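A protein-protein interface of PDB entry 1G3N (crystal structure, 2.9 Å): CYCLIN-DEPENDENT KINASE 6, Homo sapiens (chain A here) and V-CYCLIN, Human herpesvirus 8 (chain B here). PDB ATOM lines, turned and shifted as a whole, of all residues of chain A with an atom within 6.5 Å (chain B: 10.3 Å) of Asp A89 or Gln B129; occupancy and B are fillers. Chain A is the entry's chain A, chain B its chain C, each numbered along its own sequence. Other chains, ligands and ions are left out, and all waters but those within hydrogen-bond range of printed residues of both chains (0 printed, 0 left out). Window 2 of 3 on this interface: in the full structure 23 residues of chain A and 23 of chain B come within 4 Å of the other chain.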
ATOM      1  N   VAL A  47      -7.307 -22.237 -29.049  1.00  0.00           N
ATOM      2  CA  VAL A  47      -6.674 -21.767 -27.818  1.00  0.00           C
ATOM      3  C   VAL A  47      -5.569 -22.702 -27.326  1.00  0.00           C
ATOM      4  O   VAL A  47      -5.759 -23.909 -27.127  1.00  0.00           O
ATOM      5  CB  VAL A  47      -7.704 -21.557 -26.679  1.00  0.00           C
ATOM      6  CG1 VAL A  47      -7.055 -20.801 -25.536  1.00  0.00           C
ATOM      7  CG2 VAL A  47      -8.911 -20.800 -27.196  1.00  0.00           C
ATOM      8  N   GLN A  48      -4.426 -22.072 -27.099  1.00  0.00           N
ATOM      9  CA  GLN A  48      -3.177 -22.679 -26.671  1.00  0.00           C
ATOM     10  C   GLN A  48      -3.083 -22.841 -25.156  1.00  0.00           C
ATOM     11  O   GLN A  48      -3.110 -21.864 -24.413  1.00  0.00           O
ATOM     12  CB  GLN A  48      -2.026 -21.785 -27.155  1.00  0.00           C
ATOM     13  CG  GLN A  48      -2.333 -21.017 -28.472  1.00  0.00           C
ATOM     14  CD  GLN A  48      -3.473 -19.948 -28.354  1.00  0.00           C
ATOM     15  OE1 GLN A  48      -4.008 -19.471 -29.375  1.00  0.00           O
ATOM     16  NE2 GLN A  48      -3.823 -19.570 -27.119  1.00  0.00           N
ATOM     17  N   THR A  49      -2.956 -24.077 -24.696  1.00  0.00           N
ATOM     18  CA  THR A  49      -2.828 -24.347 -23.266  1.00  0.00           C
ATOM     19  C   THR A  49      -1.433 -24.015 -22.784  1.00  0.00           C
ATOM     20  O   THR A  49      -0.444 -24.351 -23.437  1.00  0.00           O
ATOM     21  CB  THR A  49      -3.024 -25.815 -22.954  1.00  0.00           C
ATOM     22  OG1 THR A  49      -4.297 -26.234 -23.452  1.00  0.00           O
ATOM     23  CG2 THR A  49      -2.927 -26.058 -21.436  1.00  0.00           C
ATOM     24  N   GLY A  50      -1.346 -23.373 -21.633  1.00  0.00           N
ATOM     25  CA  GLY A  50      -0.045 -23.042 -21.090  1.00  0.00           C
ATOM     26  C   GLY A  50       0.225 -23.917 -19.884  1.00  0.00           C
ATOM     27  O   GLY A  50      -0.559 -24.820 -19.574  1.00  0.00           O
ATOM     28  N   SER A  86     -12.140 -29.778 -26.726  1.00  0.00           N
ATOM     29  CA  SER A  86     -10.739 -30.034 -26.372  1.00  0.00           C
ATOM     30  C   SER A  86     -10.113 -31.199 -27.156  1.00  0.00           C
ATOM     31  O   SER A  86     -10.495 -32.359 -27.019  1.00  0.00           O
ATOM     32  CB  SER A  86     -10.588 -30.245 -24.852  1.00  0.00           C
ATOM     33  OG  SER A  86     -11.462 -31.250 -24.359  1.00  0.00           O
ATOM     34  N   ARG A  87      -9.145 -30.838 -27.995  1.00  0.00           N
ATOM     35  CA  ARG A  87      -8.386 -31.738 -28.867  1.00  0.00           C
ATOM     36  C   ARG A  87      -7.453 -32.612 -28.011  1.00  0.00           C
ATOM     37  O   ARG A  87      -7.763 -33.769 -27.711  1.00  0.00           O
ATOM     38  CB  ARG A  87      -7.592 -30.855 -29.845  1.00  0.00           C
ATOM     39  CG  ARG A  87      -6.941 -31.524 -31.033  1.00  0.00           C
ATOM     40  CD  ARG A  87      -6.731 -30.448 -32.113  1.00  0.00           C
ATOM     41  NE  ARG A  87      -6.178 -30.949 -33.376  1.00  0.00           N
ATOM     42  CZ  ARG A  87      -6.047 -30.212 -34.480  1.00  0.00           C
ATOM     43  NH1 ARG A  87      -6.433 -28.942 -34.476  1.00  0.00           N
ATOM     44  NH2 ARG A  87      -5.519 -30.732 -35.582  1.00  0.00           N
ATOM     45  N   THR A  88      -6.317 -32.033 -27.620  1.00  0.00           N
ATOM     46  CA  THR A  88      -5.326 -32.692 -26.769  1.00  0.00           C
ATOM     47  C   THR A  88      -5.119 -31.722 -25.595  1.00  0.00           C
ATOM     48  O   THR A  88      -6.006 -30.924 -25.282  1.00  0.00           O
ATOM     49  CB  THR A  88      -3.995 -32.874 -27.521  1.00  0.00           C
ATOM     50  OG1 THR A  88      -3.349 -31.603 -27.666  1.00  0.00           O
ATOM     51  CG2 THR A  88      -4.256 -33.452 -28.911  1.00  0.00           C
ATOM     52  N   ASP A  89      -3.981 -31.773 -24.921  1.00  0.00           N
ATOM     53  CA  ASP A  89      -3.807 -30.807 -23.852  1.00  0.00           C
ATOM     54  C   ASP A  89      -3.594 -29.457 -24.501  1.00  0.00           C
ATOM     55  O   ASP A  89      -4.430 -28.561 -24.369  1.00  0.00           O
ATOM     56  CB  ASP A  89      -2.609 -31.118 -22.950  1.00  0.00           C
ATOM     57  CG  ASP A  89      -2.929 -32.154 -21.880  1.00  0.00           C
ATOM     58  OD1 ASP A  89      -4.013 -32.054 -21.264  1.00  0.00           O
ATOM     59  OD2 ASP A  89      -2.092 -33.050 -21.628  1.00  0.00           O
ATOM     60  N   ARG A  90      -2.485 -29.329 -25.228  1.00  0.00           N
ATOM     61  CA  ARG A  90      -2.130 -28.080 -25.891  1.00  0.00           C
ATOM     62  C   ARG A  90      -3.184 -27.348 -26.747  1.00  0.00           C
ATOM     63  O   ARG A  90      -2.995 -26.171 -27.058  1.00  0.00           O
ATOM     64  CB  ARG A  90      -0.860 -28.291 -26.718  1.00  0.00           C
ATOM     65  CG  ARG A  90       0.405 -28.446 -25.895  1.00  0.00           C
ATOM     66  CD  ARG A  90       1.621 -28.277 -26.789  1.00  0.00           C
ATOM     67  NE  ARG A  90       2.806 -27.894 -26.028  1.00  0.00           N
ATOM     68  CZ  ARG A  90       3.937 -27.456 -26.579  1.00  0.00           C
ATOM     69  NH1 ARG A  90       4.035 -27.348 -27.901  1.00  0.00           N
ATOM     70  NH2 ARG A  90       4.964 -27.106 -25.808  1.00  0.00           N
ATOM     71  N   GLU A  91      -4.278 -28.013 -27.129  1.00  0.00           N
ATOM     72  CA  GLU A  91      -5.299 -27.344 -27.942  1.00  0.00           C
ATOM     73  C   GLU A  91      -6.741 -27.529 -27.538  1.00  0.00           C
ATOM     74  O   GLU A  91      -7.155 -28.616 -27.162  1.00  0.00           O
ATOM     75  CB  GLU A  91      -5.235 -27.761 -29.409  1.00  0.00           C
ATOM     76  CG  GLU A  91      -3.952 -27.470 -30.125  1.00  0.00           C
ATOM     77  CD  GLU A  91      -4.188 -27.251 -31.593  1.00  0.00           C
ATOM     78  OE1 GLU A  91      -5.100 -27.906 -32.154  1.00  0.00           O
ATOM     79  OE2 GLU A  91      -3.454 -26.427 -32.180  1.00  0.00           O
ATOM     80  N   THR A  92      -7.504 -26.447 -27.666  1.00  0.00           N
ATOM     81  CA  THR A  92      -8.935 -26.441 -27.389  1.00  0.00           C
ATOM     82  C   THR A  92      -9.586 -25.591 -28.486  1.00  0.00           C
ATOM     83  O   THR A  92      -9.191 -24.451 -28.718  1.00  0.00           O
ATOM     84  CB  THR A  92      -9.260 -25.815 -26.005  1.00  0.00           C
ATOM     85  OG1 THR A  92      -8.663 -26.602 -24.967  1.00  0.00           O
ATOM     86  CG2 THR A  92     -10.776 -25.753 -25.780  1.00  0.00           C
ATOM     87  N   LYS B  95      -9.758 -29.078  -4.505  1.00  0.00           N
ATOM     88  CA  LYS B  95      -9.193 -28.820  -5.828  1.00  0.00           C
ATOM     89  C   LYS B  95     -10.136 -27.920  -6.614  1.00  0.00           C
ATOM     90  O   LYS B  95      -9.693 -27.030  -7.347  1.00  0.00           O
ATOM     91  CB  LYS B  95      -8.999 -30.133  -6.595  1.00  0.00           C
ATOM     92  CG  LYS B  95      -8.519 -29.951  -8.019  1.00  0.00           C
ATOM     93  CD  LYS B  95      -8.193 -31.269  -8.690  1.00  0.00           C
ATOM     94  CE  LYS B  95      -9.350 -32.243  -8.705  1.00  0.00           C
ATOM     95  NZ  LYS B  95      -8.955 -33.488  -9.433  1.00  0.00           N
ATOM     96  N   ALA B  99      -9.507 -24.224  -8.315  1.00  0.00           N
ATOM     97  CA  ALA B  99      -9.754 -23.841  -9.696  1.00  0.00           C
ATOM     98  C   ALA B  99     -10.512 -22.536  -9.689  1.00  0.00           C
ATOM     99  O   ALA B  99     -10.248 -21.668 -10.505  1.00  0.00           O
ATOM    100  CB  ALA B  99     -10.554 -24.905 -10.402  1.00  0.00           C
ATOM    101  N   LEU B 102      -7.961 -19.791  -9.011  1.00  0.00           N
ATOM    102  CA  LEU B 102      -7.143 -19.578 -10.200  1.00  0.00           C
ATOM    103  C   LEU B 102      -7.941 -18.706 -11.158  1.00  0.00           C
ATOM    104  O   LEU B 102      -7.591 -17.560 -11.397  1.00  0.00           O
ATOM    105  CB  LEU B 102      -6.820 -20.936 -10.861  1.00  0.00           C
ATOM    106  CG  LEU B 102      -5.887 -21.035 -12.074  1.00  0.00           C
ATOM    107  CD1 LEU B 102      -4.549 -20.454 -11.704  1.00  0.00           C
ATOM    108  CD2 LEU B 102      -5.722 -22.490 -12.510  1.00  0.00           C
ATOM    109  N   THR B 115      -0.500 -21.728 -10.672  1.00  0.00           N
ATOM    110  CA  THR B 115      -0.933 -23.095 -10.450  1.00  0.00           C
ATOM    111  C   THR B 115      -0.067 -23.691  -9.357  1.00  0.00           C
ATOM    112  O   THR B 115      -0.566 -24.099  -8.314  1.00  0.00           O
ATOM    113  CB  THR B 115      -0.789 -23.933 -11.722  1.00  0.00           C
ATOM    114  OG1 THR B 115       0.528 -23.767 -12.247  1.00  0.00           O
ATOM    115  CG2 THR B 115      -1.790 -23.492 -12.755  1.00  0.00           C
ATOM    116  N   SER B 116       1.238 -23.732  -9.601  1.00  0.00           N
ATOM    117  CA  SER B 116       2.198 -24.278  -8.641  1.00  0.00           C
ATOM    118  C   SER B 116       1.988 -23.708  -7.237  1.00  0.00           C
ATOM    119  O   SER B 116       1.993 -24.440  -6.232  1.00  0.00           O
ATOM    120  CB  SER B 116       3.614 -23.998  -9.138  1.00  0.00           C
ATOM    121  OG  SER B 116       3.705 -22.664  -9.594  1.00  0.00           O
ATOM    122  N   CYS B 119      -1.237 -25.427  -5.920  1.00  0.00           N
ATOM    123  CA  CYS B 119      -0.985 -26.832  -5.597  1.00  0.00           C
ATOM    124  C   CYS B 119      -0.215 -26.943  -4.301  1.00  0.00           C
ATOM    125  O   CYS B 119      -0.396 -27.885  -3.525  1.00  0.00           O
ATOM    126  CB  CYS B 119      -0.174 -27.500  -6.684  1.00  0.00           C
ATOM    127  SG  CYS B 119      -1.038 -27.731  -8.176  1.00  0.00           S
ATOM    128  N   ASP B 124      -0.087 -29.885  -1.622  1.00  0.00           N
ATOM    129  CA  ASP B 124       0.329 -30.653  -2.772  1.00  0.00           C
ATOM    130  C   ASP B 124      -0.608 -31.859  -2.954  1.00  0.00           C
ATOM    131  O   ASP B 124      -0.230 -32.844  -3.573  1.00  0.00           O
ATOM    132  CB  ASP B 124       1.769 -31.117  -2.560  1.00  0.00           C
ATOM    133  CG  ASP B 124       2.342 -31.810  -3.771  1.00  0.00           C
ATOM    134  OD1 ASP B 124       2.384 -31.168  -4.853  1.00  0.00           O
ATOM    135  OD2 ASP B 124       2.750 -32.992  -3.636  1.00  0.00           O
ATOM    136  N   SER B 125      -1.831 -31.770  -2.427  1.00  0.00           N
ATOM    137  CA  SER B 125      -2.788 -32.865  -2.507  1.00  0.00           C
ATOM    138  C   SER B 125      -3.208 -33.184  -3.921  1.00  0.00           C
ATOM    139  O   SER B 125      -3.632 -34.303  -4.203  1.00  0.00           O
ATOM    140  CB  SER B 125      -4.008 -32.559  -1.659  1.00  0.00           C
ATOM    141  OG  SER B 125      -4.545 -31.311  -2.032  1.00  0.00           O
ATOM    142  N   PHE B 126      -3.115 -32.214  -4.820  1.00  0.00           N
ATOM    143  CA  PHE B 126      -3.450 -32.497  -6.206  1.00  0.00           C
ATOM    144  C   PHE B 126      -2.343 -32.002  -7.153  1.00  0.00           C
ATOM    145  O   PHE B 126      -1.557 -31.090  -6.817  1.00  0.00           O
ATOM    146  CB  PHE B 126      -4.847 -31.932  -6.581  1.00  0.00           C
ATOM    147  CG  PHE B 126      -5.004 -30.455  -6.337  1.00  0.00           C
ATOM    148  CD1 PHE B 126      -4.409 -29.527  -7.173  1.00  0.00           C
ATOM    149  CD2 PHE B 126      -5.645 -30.004  -5.194  1.00  0.00           C
ATOM    150  CE1 PHE B 126      -4.436 -28.186  -6.868  1.00  0.00           C
ATOM    151  CE2 PHE B 126      -5.677 -28.646  -4.879  1.00  0.00           C
ATOM    152  CZ  PHE B 126      -5.065 -27.734  -5.717  1.00  0.00           C
ATOM    153  N   SER B 127      -2.279 -32.643  -8.323  1.00  0.00           N
ATOM    154  CA  SER B 127      -1.293 -32.357  -9.370  1.00  0.00           C
ATOM    155  C   SER B 127      -1.553 -31.084 -10.150  1.00  0.00           C
ATOM    156  O   SER B 127      -2.693 -30.664 -10.293  1.00  0.00           O
ATOM    157  CB  SER B 127      -1.266 -33.525 -10.354  1.00  0.00           C
ATOM    158  OG  SER B 127      -0.521 -33.208 -11.512  1.00  0.00           O
ATOM    159  N   ARG B 128      -0.496 -30.472 -10.669  1.00  0.00           N
ATOM    160  CA  ARG B 128      -0.673 -29.272 -11.477  1.00  0.00           C
ATOM    161  C   ARG B 128      -1.591 -29.584 -12.677  1.00  0.00           C
ATOM    162  O   ARG B 128      -2.442 -28.787 -13.045  1.00  0.00           O
ATOM    163  CB  ARG B 128       0.687 -28.732 -11.953  1.00  0.00           C
ATOM    164  CG  ARG B 128       0.588 -27.806 -13.178  1.00  0.00           C
ATOM    165  CD  ARG B 128       1.927 -27.167 -13.615  1.00  0.00           C
ATOM    166  NE  ARG B 128       2.316 -26.030 -12.770  1.00  0.00           N
ATOM    167  CZ  ARG B 128       3.335 -25.199 -13.017  1.00  0.00           C
ATOM    168  NH1 ARG B 128       4.099 -25.358 -14.091  1.00  0.00           N
ATOM    169  NH2 ARG B 128       3.573 -24.177 -12.203  1.00  0.00           N
ATOM    170  N   GLN B 129      -1.429 -30.744 -13.291  1.00  0.00           N
ATOM    171  CA  GLN B 129      -2.296 -31.081 -14.407  1.00  0.00           C
ATOM    172  C   GLN B 129      -3.734 -31.116 -13.950  1.00  0.00           C
ATOM    173  O   GLN B 129      -4.612 -30.519 -14.562  1.00  0.00           O
ATOM    174  CB  GLN B 129      -1.948 -32.447 -14.989  1.00  0.00           C
ATOM    175  CG  GLN B 129      -0.961 -32.406 -16.131  1.00  0.00           C
ATOM    176  CD  GLN B 129      -1.413 -31.487 -17.260  1.00  0.00           C
ATOM    177  OE1 GLN B 129      -2.559 -31.566 -17.741  1.00  0.00           O
ATOM    178  NE2 GLN B 129      -0.505 -30.616 -17.697  1.00  0.00           N
ATOM    179  N   GLU B 130      -3.949 -31.843 -12.863  1.00  0.00           N
ATOM    180  CA  GLU B 130      -5.262 -32.030 -12.266  1.00  0.00           C
ATOM    181  C   GLU B 130      -5.986 -30.746 -11.922  1.00  0.00           C
ATOM    182  O   GLU B 130      -7.211 -30.694 -12.013  1.00  0.00           O
ATOM    183  CB  GLU B 130      -5.125 -32.887 -11.025  1.00  0.00           C
ATOM    184  CG  GLU B 130      -4.652 -34.293 -11.297  1.00  0.00           C
ATOM    185  CD  GLU B 130      -4.355 -35.015 -10.008  1.00  0.00           C
ATOM    186  OE1 GLU B 130      -5.181 -34.915  -9.070  1.00  0.00           O
ATOM    187  OE2 GLU B 130      -3.310 -35.685  -9.929  1.00  0.00           O
ATOM    188  N   LEU B 131      -5.242 -29.723 -11.514  1.00  0.00           N
ATOM    189  CA  LEU B 131      -5.857 -28.439 -11.194  1.00  0.00           C
ATOM    190  C   LEU B 131      -6.265 -27.780 -12.486  1.00  0.00           C
ATOM    191  O   LEU B 131      -7.311 -27.132 -12.559  1.00  0.00           O
ATOM    192  CB  LEU B 131      -4.887 -27.516 -10.472  1.00  0.00           C
ATOM    193  CG  LEU B 131      -5.451 -26.110 -10.292  1.00  0.00           C
ATOM    194  CD1 LEU B 131      -6.772 -26.179  -9.552  1.00  0.00           C
ATOM    195  CD2 LEU B 131      -4.440 -25.263  -9.550  1.00  0.00           C
ATOM    196  N   ILE B 132      -5.416 -27.950 -13.500  1.00  0.00           N
ATOM    197  CA  ILE B 132      -5.640 -27.401 -14.839  1.00  0.00           C
ATOM    198  C   ILE B 132      -6.848 -28.038 -15.489  1.00  0.00           C
ATOM    199  O   ILE B 132      -7.594 -27.378 -16.197  1.00  0.00           O
ATOM    200  CB  ILE B 132      -4.401 -27.622 -15.744  1.00  0.00           C
ATOM    201  CG1 ILE B 132      -3.269 -26.713 -15.284  1.00  0.00           C
ATOM    202  CG2 ILE B 132      -4.728 -27.330 -17.168  1.00  0.00           C
ATOM    203  CD1 ILE B 132      -2.045 -26.788 -16.119  1.00  0.00           C
ATOM    204  N   ASP B 133      -7.026 -29.327 -15.228  1.00  0.00           N
ATOM    205  CA  ASP B 133      -8.129 -30.085 -15.780  1.00  0.00           C
ATOM    206  C   ASP B 133      -9.424 -29.691 -15.096  1.00  0.00           C
ATOM    207  O   ASP B 133     -10.519 -29.880 -15.635  1.00  0.00           O
ATOM    208  CB  ASP B 133      -7.861 -31.584 -15.634  1.00  0.00           C
ATOM    209  CG  ASP B 133      -6.661 -32.057 -16.466  1.00  0.00           C
ATOM    210  OD1 ASP B 133      -6.678 -31.917 -17.720  1.00  0.00           O
ATOM    211  OD2 ASP B 133      -5.698 -32.571 -15.860  1.00  0.00           O
ATOM    212  N   GLN B 134      -9.302 -29.146 -13.897  1.00  0.00           N
ATOM    213  CA  GLN B 134     -10.475 -28.687 -13.183  1.00  0.00           C
ATOM    214  C   GLN B 134     -10.819 -27.298 -13.677  1.00  0.00           C
ATOM    215  O   GLN B 134     -11.978 -26.899 -13.665  1.00  0.00           O
ATOM    216  CB  GLN B 134     -10.222 -28.662 -11.683  1.00  0.00           C
ATOM    217  CG  GLN B 134     -10.404 -30.010 -11.015  1.00  0.00           C
ATOM    218  CD  GLN B 134     -11.846 -30.500 -11.049  1.00  0.00           C
ATOM    219  OE1 GLN B 134     -12.765 -29.816 -10.591  1.00  0.00           O
ATOM    220  NE2 GLN B 134     -12.045 -31.695 -11.588  1.00  0.00           N
ATOM    221  N   GLU B 135      -9.812 -26.552 -14.108  1.00  0.00           N
ATOM    222  CA  GLU B 135     -10.085 -25.229 -14.623  1.00  0.00           C
ATOM    223  C   GLU B 135     -10.862 -25.392 -15.916  1.00  0.00           C
ATOM    224  O   GLU B 135     -11.844 -24.687 -16.134  1.00  0.00           O
ATOM    225  CB  GLU B 135      -8.804 -24.475 -14.934  1.00  0.00           C
ATOM    226  CG  GLU B 135      -9.020 -22.991 -15.228  1.00  0.00           C
ATOM    227  CD  GLU B 135      -7.748 -22.333 -15.718  1.00  0.00           C
ATOM    228  OE1 GLU B 135      -7.573 -21.105 -15.526  1.00  0.00           O
ATOM    229  OE2 GLU B 135      -6.924 -23.063 -16.322  1.00  0.00           O
ATOM    230  N   LYS B 136     -10.415 -26.320 -16.766  1.00  0.00           N
ATOM    231  CA  LYS B 136     -11.071 -26.562 -18.043  1.00  0.00           C
ATOM    232  C   LYS B 136     -12.518 -27.002 -17.772  1.00  0.00           C
ATOM    233  O   LYS B 136     -13.485 -26.560 -18.427  1.00  0.00           O
ATOM    234  CB  LYS B 136     -10.297 -27.633 -18.847  1.00  0.00           C
ATOM    235  CG  LYS B 136     -10.942 -27.965 -20.213  1.00  0.00           C
ATOM    236  CD  LYS B 136     -10.210 -29.004 -21.098  1.00  0.00           C
ATOM    237  CE  LYS B 136      -8.938 -28.440 -21.743  1.00  0.00           C
ATOM    238  NZ  LYS B 136      -8.313 -29.332 -22.796  1.00  0.00           N
ATOM    239  N   GLU B 137     -12.639 -27.846 -16.757  1.00  0.00           N
ATOM    240  CA  GLU B 137     -13.906 -28.417 -16.314  1.00  0.00           C
ATOM    241  C   GLU B 137     -14.844 -27.323 -15.845  1.00  0.00           C
ATOM    242  O   GLU B 137     -15.993 -27.257 -16.270  1.00  0.00           O
ATOM    243  CB  GLU B 137     -13.619 -29.397 -15.177  1.00  0.00           C
ATOM    244  CG  GLU B 137     -14.296 -30.754 -15.292  1.00  0.00           C
ATOM    245  CD  GLU B 137     -15.780 -30.673 -15.074  1.00  0.00           C
ATOM    246  OE1 GLU B 137     -16.476 -31.714 -15.124  1.00  0.00           O
ATOM    247  OE2 GLU B 137     -16.251 -29.545 -14.848  1.00  0.00           O
ATOM    248  N   GLU B 140     -16.116 -25.263 -18.609  1.00  0.00           N
ATOM    249  CA  GLU B 140     -17.116 -25.943 -19.395  1.00  0.00           C
ATOM    250  C   GLU B 140     -18.482 -26.015 -18.732  1.00  0.00           C
ATOM    251  O   GLU B 140     -19.485 -25.774 -19.389  1.00  0.00           O
ATOM    252  CB  GLU B 140     -16.633 -27.331 -19.770  1.00  0.00           C
ATOM    253  CG  GLU B 140     -15.417 -27.273 -20.662  1.00  0.00           C
ATOM    254  CD  GLU B 140     -15.152 -28.580 -21.392  1.00  0.00           C
ATOM    255  OE1 GLU B 140     -14.184 -28.641 -22.194  1.00  0.00           O
ATOM    256  OE2 GLU B 140     -15.921 -29.545 -21.168  1.00  0.00           O
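The backbone carbonyl oxygen (O) of Thr A92 is in hydrogen-bond range of the backbone NH (N) of Val A47, 2.9 Å away.
OG1 of Thr A49 sits at hydrogen-bond distance from O of Asp A89 (2.5 Å).
OG1 of Thr A88 sits at hydrogen-bond distance from N of Arg A90 (3.4 Å).
The side-chain hydroxyl of Ser B127 sits close to the backbone NH of Gln B129, 3.2 Å away.
O of Gln B129 sits close to OD2 of Asp B133 (2.7 Å).
CB of Ser A86 touches NZ of Lys B136, 3.2 Å away.
O of Thr A88 touches NZ of Lys B136 (3.7 Å).
Gln B129 touches Asp A89.
NZ of Lys B136 touches OG1 of Thr A92, 3.5 Å away.
Printed residues of chain A that touch a printed residue of chain B: Ser A86, Thr A88, Asp A89 and Thr A92.
Printed residues of chain B that touch a printed residue of chain A: Gln B129 and Lys B136.
Among the printed residues, 4 pairs touch across the chains.
Asp A89 touches just one residue of chain B: Gln B129 (3.8 Å).
Gln B129 touches just one residue of chain A: Asp A89.
No residue of chain B comes within 4 Å of Thr A49.
Of the printed residues of chain B, Thr A88 touches Lys B136.
Of the printed residues of chain B, Ser A86 touches Lys B136 (3.2 Å).
Of the printed residues of chain A, Lys B136 touches Ser A86 (3.2 Å), Thr A88 (3.7 Å) and Thr A92 (3.5 Å).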
